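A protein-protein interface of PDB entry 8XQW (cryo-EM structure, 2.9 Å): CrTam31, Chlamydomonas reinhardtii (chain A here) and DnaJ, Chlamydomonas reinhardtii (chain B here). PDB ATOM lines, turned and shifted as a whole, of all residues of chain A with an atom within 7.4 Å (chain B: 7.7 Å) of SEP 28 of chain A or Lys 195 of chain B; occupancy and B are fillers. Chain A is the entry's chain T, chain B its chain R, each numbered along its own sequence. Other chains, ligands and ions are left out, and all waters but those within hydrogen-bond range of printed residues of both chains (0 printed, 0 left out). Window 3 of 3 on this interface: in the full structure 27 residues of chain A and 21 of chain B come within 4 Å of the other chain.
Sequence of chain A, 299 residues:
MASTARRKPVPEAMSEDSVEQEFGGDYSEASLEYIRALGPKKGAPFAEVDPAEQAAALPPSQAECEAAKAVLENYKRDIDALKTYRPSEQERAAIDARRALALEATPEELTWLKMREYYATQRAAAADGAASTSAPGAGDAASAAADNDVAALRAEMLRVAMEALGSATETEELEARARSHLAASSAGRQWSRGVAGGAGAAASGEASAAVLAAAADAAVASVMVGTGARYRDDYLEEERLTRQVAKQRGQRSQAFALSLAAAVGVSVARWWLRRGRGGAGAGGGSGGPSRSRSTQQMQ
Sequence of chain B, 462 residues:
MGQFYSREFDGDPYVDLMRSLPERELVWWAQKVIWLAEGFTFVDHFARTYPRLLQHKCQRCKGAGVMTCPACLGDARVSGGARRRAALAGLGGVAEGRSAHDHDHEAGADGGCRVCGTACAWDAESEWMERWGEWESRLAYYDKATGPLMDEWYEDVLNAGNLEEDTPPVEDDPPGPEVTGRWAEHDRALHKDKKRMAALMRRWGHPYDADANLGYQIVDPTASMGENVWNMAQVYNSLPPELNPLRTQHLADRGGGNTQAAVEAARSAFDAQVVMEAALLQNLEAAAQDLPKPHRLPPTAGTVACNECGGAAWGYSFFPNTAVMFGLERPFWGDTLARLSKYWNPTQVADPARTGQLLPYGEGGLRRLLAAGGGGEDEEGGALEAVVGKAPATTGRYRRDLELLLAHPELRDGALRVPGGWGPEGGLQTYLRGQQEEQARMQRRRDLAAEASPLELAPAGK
O2P of SEP 28 of chain A sits close to the side-chain amino group of Lys 192 of chain B. The side-chain hydroxyl (OH) of Tyr 27 of chain A lies within hydrogen-bond range of the backbone carbonyl oxygen (O) of Lys 195 of chain B, at 2.7 Å. The side-chain amino group (NZ) of Lys 195 of chain B sits close to O3P of SEP 28 of chain A (3.99 Å). The guanidinium group of Arg 196 of chain B is in hydrogen-bond range of the side-chain hydroxyl of Ser 31 of chain A (3.0 Å).
OG of SEP 28 of chain A lies within hydrogen-bond range of N of Ala 30 of chain A, 3.3 Å away. O2P of SEP 28 of chain A lies within hydrogen-bond range of OG of Ser 31 of chain A (3.0 Å).
CB of Ala 199 of chain B touches CE1 of Phe 23 of chain A, 3.6 Å away. Phe 23 of chain A touches Arg 202 of chain B (CE1 to CZ, 3.99 Å). Tyr 27 of chain A touches Ala 199 of chain B. Lys 192 of chain B touches Ala 30 of chain A. Ala 30 of chain A touches Arg 196 of chain B.
Of the printed residues of chain B, SEP 28 of chain A touches Lys 192 and Lys 195. Printed residues of chain A within 4 Å of Lys 192 of chain B: SEP 28 and Ala 30. Of the printed residues of chain B, Ala 30 of chain A touches Lys 192 (3.4 Å) and Arg 196 (3.2 Å). Gly 24 of chain A touches none of the printed residues of chain B. The nearest printed residue of chain B that does not touch Ser 31 of chain A is Lys 192 of chain B (4.6 Å).
Of the 13 printed residues of chain A, 5 touch a printed residue of chain B. Of the 13 printed residues of chain B, 5 touch a printed residue of chain A. Hydrophobic or aromatic side chains of chain B within 4 Å of the printed part of chain A: Ala 199.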
ATOM      1  N   PHE A  23      15.218  29.822  15.075  1.00  0.00           N
ATOM      2  CA  PHE A  23      15.126  28.688  15.985  1.00  0.00           C
ATOM      3  C   PHE A  23      15.525  29.031  17.411  1.00  0.00           C
ATOM      4  O   PHE A  23      14.709  28.864  18.322  1.00  0.00           O
ATOM      5  CB  PHE A  23      15.993  27.533  15.474  1.00  0.00           C
ATOM      6  CG  PHE A  23      15.598  27.045  14.110  1.00  0.00           C
ATOM      7  CD1 PHE A  23      14.605  26.097  13.962  1.00  0.00           C
ATOM      8  CD2 PHE A  23      16.212  27.546  12.976  1.00  0.00           C
ATOM      9  CE1 PHE A  23      14.235  25.653  12.711  1.00  0.00           C
ATOM     10  CE2 PHE A  23      15.845  27.105  11.725  1.00  0.00           C
ATOM     11  CZ  PHE A  23      14.856  26.159  11.593  1.00  0.00           C
ATOM     12  N   GLY A  24      16.749  29.512  17.620  1.00  0.00           N
ATOM     13  CA  GLY A  24      17.208  29.965  18.920  1.00  0.00           C
ATOM     14  C   GLY A  24      16.940  29.031  20.084  1.00  0.00           C
ATOM     15  O   GLY A  24      17.329  27.861  20.062  1.00  0.00           O
ATOM     16  N   GLY A  25      16.258  29.546  21.105  1.00  0.00           N
ATOM     17  CA  GLY A  25      16.016  28.798  22.324  1.00  0.00           C
ATOM     18  C   GLY A  25      15.070  27.629  22.197  1.00  0.00           C
ATOM     19  O   GLY A  25      14.870  26.905  23.177  1.00  0.00           O
ATOM     20  N   ASP A  26      14.479  27.423  21.018  1.00  0.00           N
ATOM     21  CA  ASP A  26      13.647  26.247  20.802  1.00  0.00           C
ATOM     22  C   ASP A  26      14.467  24.967  20.784  1.00  0.00           C
ATOM     23  O   ASP A  26      13.898  23.876  20.901  1.00  0.00           O
ATOM     24  CB  ASP A  26      12.869  26.388  19.497  1.00  0.00           C
ATOM     25  CG  ASP A  26      11.469  26.920  19.709  1.00  0.00           C
ATOM     26  OD1 ASP A  26      10.804  26.477  20.670  1.00  0.00           O
ATOM     27  OD2 ASP A  26      11.035  27.784  18.919  1.00  0.00           O
ATOM     28  N   TYR A  27      15.783  25.078  20.638  1.00  0.00           N
ATOM     29  CA  TYR A  27      16.675  23.934  20.678  1.00  0.00           C
ATOM     30  C   TYR A  27      17.908  24.302  21.490  1.00  0.00           C
ATOM     31  O   TYR A  27      18.128  25.474  21.793  1.00  0.00           O
ATOM     32  CB  TYR A  27      17.075  23.506  19.266  1.00  0.00           C
ATOM     33  CG  TYR A  27      15.924  23.128  18.362  1.00  0.00           C
ATOM     34  CD1 TYR A  27      15.267  24.086  17.605  1.00  0.00           C
ATOM     35  CD2 TYR A  27      15.505  21.810  18.255  1.00  0.00           C
ATOM     36  CE1 TYR A  27      14.219  23.746  16.775  1.00  0.00           C
ATOM     37  CE2 TYR A  27      14.460  21.459  17.427  1.00  0.00           C
ATOM     38  CZ  TYR A  27      13.819  22.431  16.687  1.00  0.00           C
ATOM     39  OH  TYR A  27      12.775  22.088  15.860  1.00  0.00           O
ATOM     40  N   SEP A  28      18.716  23.307  21.836  1.00  0.00           N
ATOM     41  CA  SEP A  28      19.957  23.549  22.564  1.00  0.00           C
ATOM     42  CB  SEP A  28      20.445  22.269  23.236  1.00  0.00           C
ATOM     43  OG  SEP A  28      20.546  21.223  22.293  1.00  0.00           O
ATOM     44  C   SEP A  28      21.029  24.082  21.634  1.00  0.00           C
ATOM     45  O   SEP A  28      20.736  24.781  20.671  1.00  0.00           O
ATOM     46  P   SEP A  28      19.346  20.190  22.550  1.00  0.00           P
ATOM     47  O1P SEP A  28      19.700  19.306  23.844  1.00  0.00           O
ATOM     48  O2P SEP A  28      19.149  19.242  21.264  1.00  0.00           O
ATOM     49  O3P SEP A  28      17.987  21.012  22.803  1.00  0.00           O
ATOM     50  N   GLU A  29      22.279  23.753  21.931  1.00  0.00           N
ATOM     51  CA  GLU A  29      23.372  24.091  21.031  1.00  0.00           C
ATOM     52  C   GLU A  29      23.651  22.917  20.110  1.00  0.00           C
ATOM     53  O   GLU A  29      24.192  23.081  19.018  1.00  0.00           O
ATOM     54  CB  GLU A  29      24.630  24.470  21.808  1.00  0.00           C
ATOM     55  CG  GLU A  29      24.857  25.965  21.887  1.00  0.00           C
ATOM     56  CD  GLU A  29      24.697  26.646  20.543  1.00  0.00           C
ATOM     57  OE1 GLU A  29      25.632  26.576  19.720  1.00  0.00           O
ATOM     58  OE2 GLU A  29      23.633  27.251  20.307  1.00  0.00           O
ATOM     59  N   ALA A  30      23.272  21.724  20.570  1.00  0.00           N
ATOM     60  CA  ALA A  30      23.450  20.527  19.757  1.00  0.00           C
ATOM     61  C   ALA A  30      22.678  20.633  18.451  1.00  0.00           C
ATOM     62  O   ALA A  30      23.253  20.479  17.368  1.00  0.00           O
ATOM     63  CB  ALA A  30      23.011  19.292  20.540  1.00  0.00           C
ATOM     64  N   SER A  31      21.378  20.910  18.530  1.00  0.00           N
ATOM     65  CA  SER A  31      20.578  21.005  17.317  1.00  0.00           C
ATOM     66  C   SER A  31      20.942  22.236  16.500  1.00  0.00           C
ATOM     67  O   SER A  31      20.768  22.241  15.273  1.00  0.00           O
ATOM     68  CB  SER A  31      19.098  21.006  17.673  1.00  0.00           C
ATOM     69  OG  SER A  31      18.743  19.788  18.299  1.00  0.00           O
ATOM     70  N   LEU A  32      21.487  23.271  17.137  1.00  0.00           N
ATOM     71  CA  LEU A  32      21.877  24.452  16.378  1.00  0.00           C
ATOM     72  C   LEU A  32      23.100  24.163  15.515  1.00  0.00           C
ATOM     73  O   LEU A  32      23.125  24.513  14.331  1.00  0.00           O
ATOM     74  CB  LEU A  32      22.126  25.624  17.323  1.00  0.00           C
ATOM     75  CG  LEU A  32      21.530  26.948  16.842  1.00  0.00           C
ATOM     76  CD1 LEU A  32      21.439  27.952  17.977  1.00  0.00           C
ATOM     77  CD2 LEU A  32      22.319  27.522  15.688  1.00  0.00           C
ATOM     78  N   GLU A  33      24.115  23.505  16.078  1.00  0.00           N
ATOM     79  CA  GLU A  33      25.242  23.069  15.258  1.00  0.00           C
ATOM     80  C   GLU A  33      24.815  22.009  14.256  1.00  0.00           C
ATOM     81  O   GLU A  33      25.371  21.933  13.156  1.00  0.00           O
ATOM     82  CB  GLU A  33      26.368  22.539  16.143  1.00  0.00           C
ATOM     83  CG  GLU A  33      26.918  23.575  17.095  1.00  0.00           C
ATOM     84  CD  GLU A  33      26.863  24.968  16.510  1.00  0.00           C
ATOM     85  OE1 GLU A  33      27.725  25.294  15.668  1.00  0.00           O
ATOM     86  OE2 GLU A  33      25.952  25.736  16.887  1.00  0.00           O
ATOM     87  N   ILE A  35      22.028  22.074  12.625  1.00  0.00           N
ATOM     88  CA  ILE A  35      21.496  22.815  11.485  1.00  0.00           C
ATOM     89  C   ILE A  35      22.583  23.643  10.800  1.00  0.00           C
ATOM     90  O   ILE A  35      22.494  23.921   9.599  1.00  0.00           O
ATOM     91  CB  ILE A  35      20.311  23.689  11.940  1.00  0.00           C
ATOM     92  CG1 ILE A  35      19.144  22.815  12.401  1.00  0.00           C
ATOM     93  CG2 ILE A  35      19.827  24.600  10.830  1.00  0.00           C
ATOM     94  CD1 ILE A  35      18.891  21.616  11.517  1.00  0.00           C
ATOM     95  N   ARG A  36      23.624  24.038  11.532  1.00  0.00           N
ATOM     96  CA  ARG A  36      24.623  24.939  10.968  1.00  0.00           C
ATOM     97  C   ARG A  36      25.546  24.267   9.959  1.00  0.00           C
ATOM     98  O   ARG A  36      26.199  24.969   9.184  1.00  0.00           O
ATOM     99  CB  ARG A  36      25.472  25.554  12.078  1.00  0.00           C
ATOM    100  CG  ARG A  36      24.960  26.874  12.619  1.00  0.00           C
ATOM    101  CD  ARG A  36      25.556  27.134  13.991  1.00  0.00           C
ATOM    102  NE  ARG A  36      25.285  28.481  14.479  1.00  0.00           N
ATOM    103  CZ  ARG A  36      25.485  28.871  15.733  1.00  0.00           C
ATOM    104  NH1 ARG A  36      25.949  28.017  16.631  1.00  0.00           N
ATOM    105  NH2 ARG A  36      25.212  30.114  16.094  1.00  0.00           N
ATOM    106  N   ARG B 188      21.478   9.421  23.224  1.00  0.00           N
ATOM    107  CA  ARG B 188      20.940  10.760  23.408  1.00  0.00           C
ATOM    108  C   ARG B 188      20.732  11.458  22.075  1.00  0.00           C
ATOM    109  O   ARG B 188      19.677  12.054  21.838  1.00  0.00           O
ATOM    110  CB  ARG B 188      21.867  11.581  24.299  1.00  0.00           C
ATOM    111  CG  ARG B 188      21.806  11.211  25.765  1.00  0.00           C
ATOM    112  CD  ARG B 188      22.342  12.333  26.632  1.00  0.00           C
ATOM    113  NE  ARG B 188      23.801  12.337  26.673  1.00  0.00           N
ATOM    114  CZ  ARG B 188      24.564  13.104  25.904  1.00  0.00           C
ATOM    115  NH1 ARG B 188      24.009  13.935  25.034  1.00  0.00           N
ATOM    116  NH2 ARG B 188      25.884  13.045  26.006  1.00  0.00           N
ATOM    117  N   HIS B 191      17.689   9.825  20.215  1.00  0.00           N
ATOM    118  CA  HIS B 191      16.327  10.054  20.684  1.00  0.00           C
ATOM    119  C   HIS B 191      15.794  11.435  20.334  1.00  0.00           C
ATOM    120  O   HIS B 191      14.587  11.578  20.115  1.00  0.00           O
ATOM    121  CB  HIS B 191      16.251   9.828  22.190  1.00  0.00           C
ATOM    122  CG  HIS B 191      16.125   8.386  22.565  1.00  0.00           C
ATOM    123  ND1 HIS B 191      14.909   7.743  22.644  1.00  0.00           N
ATOM    124  CD2 HIS B 191      17.065   7.457  22.862  1.00  0.00           C
ATOM    125  CE1 HIS B 191      15.104   6.482  22.984  1.00  0.00           C
ATOM    126  NE2 HIS B 191      16.401   6.283  23.124  1.00  0.00           N
ATOM    127  N   LYS B 192      16.650  12.447  20.252  1.00  0.00           N
ATOM    128  CA  LYS B 192      16.224  13.767  19.793  1.00  0.00           C
ATOM    129  C   LYS B 192      15.986  13.759  18.289  1.00  0.00           C
ATOM    130  O   LYS B 192      16.610  14.491  17.523  1.00  0.00           O
ATOM    131  CB  LYS B 192      17.263  14.810  20.180  1.00  0.00           C
ATOM    132  CG  LYS B 192      17.810  14.625  21.577  1.00  0.00           C
ATOM    133  CD  LYS B 192      18.564  15.852  22.046  1.00  0.00           C
ATOM    134  CE  LYS B 192      19.821  16.062  21.234  1.00  0.00           C
ATOM    135  NZ  LYS B 192      20.570  17.268  21.683  1.00  0.00           N
ATOM    136  N   ASP B 193      15.046  12.917  17.863  1.00  0.00           N
ATOM    137  CA  ASP B 193      14.867  12.578  16.460  1.00  0.00           C
ATOM    138  C   ASP B 193      13.765  13.375  15.777  1.00  0.00           C
ATOM    139  O   ASP B 193      13.804  13.539  14.553  1.00  0.00           O
ATOM    140  CB  ASP B 193      14.569  11.082  16.321  1.00  0.00           C
ATOM    141  CG  ASP B 193      13.314  10.660  17.084  1.00  0.00           C
ATOM    142  OD1 ASP B 193      12.621  11.536  17.644  1.00  0.00           O
ATOM    143  OD2 ASP B 193      13.017   9.446  17.121  1.00  0.00           O
ATOM    144  N   LYS B 194      12.783  13.870  16.525  1.00  0.00           N
ATOM    145  CA  LYS B 194      11.610  14.453  15.891  1.00  0.00           C
ATOM    146  C   LYS B 194      11.707  15.969  15.829  1.00  0.00           C
ATOM    147  O   LYS B 194      11.298  16.581  14.840  1.00  0.00           O
ATOM    148  CB  LYS B 194      10.353  14.019  16.638  1.00  0.00           C
ATOM    149  CG  LYS B 194       9.343  13.292  15.780  1.00  0.00           C
ATOM    150  CD  LYS B 194       8.431  12.448  16.652  1.00  0.00           C
ATOM    151  CE  LYS B 194       8.863  10.992  16.661  1.00  0.00           C
ATOM    152  NZ  LYS B 194       8.125  10.191  17.676  1.00  0.00           N
ATOM    153  N   LYS B 195      12.246  16.592  16.876  1.00  0.00           N
ATOM    154  CA  LYS B 195      12.413  18.041  16.855  1.00  0.00           C
ATOM    155  C   LYS B 195      13.479  18.467  15.853  1.00  0.00           C
ATOM    156  O   LYS B 195      13.320  19.487  15.171  1.00  0.00           O
ATOM    157  CB  LYS B 195      12.755  18.549  18.253  1.00  0.00           C
ATOM    158  CG  LYS B 195      13.645  17.619  19.056  1.00  0.00           C
ATOM    159  CD  LYS B 195      14.201  18.330  20.275  1.00  0.00           C
ATOM    160  CE  LYS B 195      14.758  17.347  21.284  1.00  0.00           C
ATOM    161  NZ  LYS B 195      15.349  18.044  22.456  1.00  0.00           N
ATOM    162  N   ARG B 196      14.557  17.690  15.733  1.00  0.00           N
ATOM    163  CA  ARG B 196      15.584  18.002  14.747  1.00  0.00           C
ATOM    164  C   ARG B 196      15.048  17.858  13.331  1.00  0.00           C
ATOM    165  O   ARG B 196      15.260  18.737  12.488  1.00  0.00           O
ATOM    166  CB  ARG B 196      16.800  17.107  14.966  1.00  0.00           C
ATOM    167  CG  ARG B 196      17.762  17.636  16.010  1.00  0.00           C
ATOM    168  CD  ARG B 196      18.851  16.635  16.320  1.00  0.00           C
ATOM    169  NE  ARG B 196      19.825  17.175  17.261  1.00  0.00           N
ATOM    170  CZ  ARG B 196      20.826  16.479  17.784  1.00  0.00           C
ATOM    171  NH1 ARG B 196      20.990  15.204  17.465  1.00  0.00           N
ATOM    172  NH2 ARG B 196      21.664  17.055  18.629  1.00  0.00           N
ATOM    173  N   MET B 197      14.348  16.757  13.051  1.00  0.00           N
ATOM    174  CA  MET B 197      13.741  16.586  11.736  1.00  0.00           C
ATOM    175  C   MET B 197      12.706  17.669  11.468  1.00  0.00           C
ATOM    176  O   MET B 197      12.534  18.107  10.325  1.00  0.00           O
ATOM    177  CB  MET B 197      13.107  15.202  11.630  1.00  0.00           C
ATOM    178  CG  MET B 197      12.282  14.995  10.376  1.00  0.00           C
ATOM    179  SD  MET B 197      13.163  15.458   8.874  1.00  0.00           S
ATOM    180  CE  MET B 197      12.377  14.395   7.670  1.00  0.00           C
ATOM    181  N   ALA B 198      12.016  18.124  12.512  1.00  0.00           N
ATOM    182  CA  ALA B 198      11.071  19.219  12.345  1.00  0.00           C
ATOM    183  C   ALA B 198      11.786  20.498  11.939  1.00  0.00           C
ATOM    184  O   ALA B 198      11.321  21.222  11.052  1.00  0.00           O
ATOM    185  CB  ALA B 198      10.285  19.428  13.635  1.00  0.00           C
ATOM    186  N   ALA B 199      12.919  20.791  12.575  1.00  0.00           N
ATOM    187  CA  ALA B 199      13.696  21.965  12.188  1.00  0.00           C
ATOM    188  C   ALA B 199      14.191  21.839  10.756  1.00  0.00           C
ATOM    189  O   ALA B 199      14.217  22.820  10.001  1.00  0.00           O
ATOM    190  CB  ALA B 199      14.867  22.158  13.149  1.00  0.00           C
ATOM    191  N   LEU B 200      14.596  20.630  10.366  1.00  0.00           N
ATOM    192  CA  LEU B 200      15.013  20.391   8.988  1.00  0.00           C
ATOM    193  C   LEU B 200      13.879  20.672   8.015  1.00  0.00           C
ATOM    194  O   LEU B 200      14.083  21.307   6.974  1.00  0.00           O
ATOM    195  CB  LEU B 200      15.501  18.954   8.829  1.00  0.00           C
ATOM    196  CG  LEU B 200      16.958  18.676   9.169  1.00  0.00           C
ATOM    197  CD1 LEU B 200      17.083  17.337   9.850  1.00  0.00           C
ATOM    198  CD2 LEU B 200      17.774  18.692   7.902  1.00  0.00           C
ATOM    199  N   MET B 201      12.673  20.202   8.335  1.00  0.00           N
ATOM    200  CA  MET B 201      11.521  20.472   7.486  1.00  0.00           C
ATOM    201  C   MET B 201      11.203  21.961   7.446  1.00  0.00           C
ATOM    202  O   MET B 201      10.714  22.473   6.434  1.00  0.00           O
ATOM    203  CB  MET B 201      10.311  19.686   7.981  1.00  0.00           C
ATOM    204  CG  MET B 201       9.281  19.412   6.913  1.00  0.00           C
ATOM    205  SD  MET B 201       9.505  17.799   6.162  1.00  0.00           S
ATOM    206  CE  MET B 201       8.586  18.002   4.643  1.00  0.00           C
ATOM    207  N   ARG B 202      11.463  22.668   8.546  1.00  0.00           N
ATOM    208  CA  ARG B 202      11.132  24.088   8.600  1.00  0.00           C
ATOM    209  C   ARG B 202      12.117  24.919   7.793  1.00  0.00           C
ATOM    210  O   ARG B 202      11.739  25.937   7.202  1.00  0.00           O
ATOM    211  CB  ARG B 202      11.090  24.562  10.051  1.00  0.00           C
ATOM    212  CG  ARG B 202       9.727  24.397  10.708  1.00  0.00           C
ATOM    213  CD  ARG B 202       9.760  24.762  12.182  1.00  0.00           C
ATOM    214  NE  ARG B 202      10.170  26.144  12.397  1.00  0.00           N
ATOM    215  CZ  ARG B 202      10.473  26.654  13.586  1.00  0.00           C
ATOM    216  NH1 ARG B 202      10.418  25.890  14.667  1.00  0.00           N
ATOM    217  NH2 ARG B 202      10.839  27.922  13.694  1.00  0.00           N
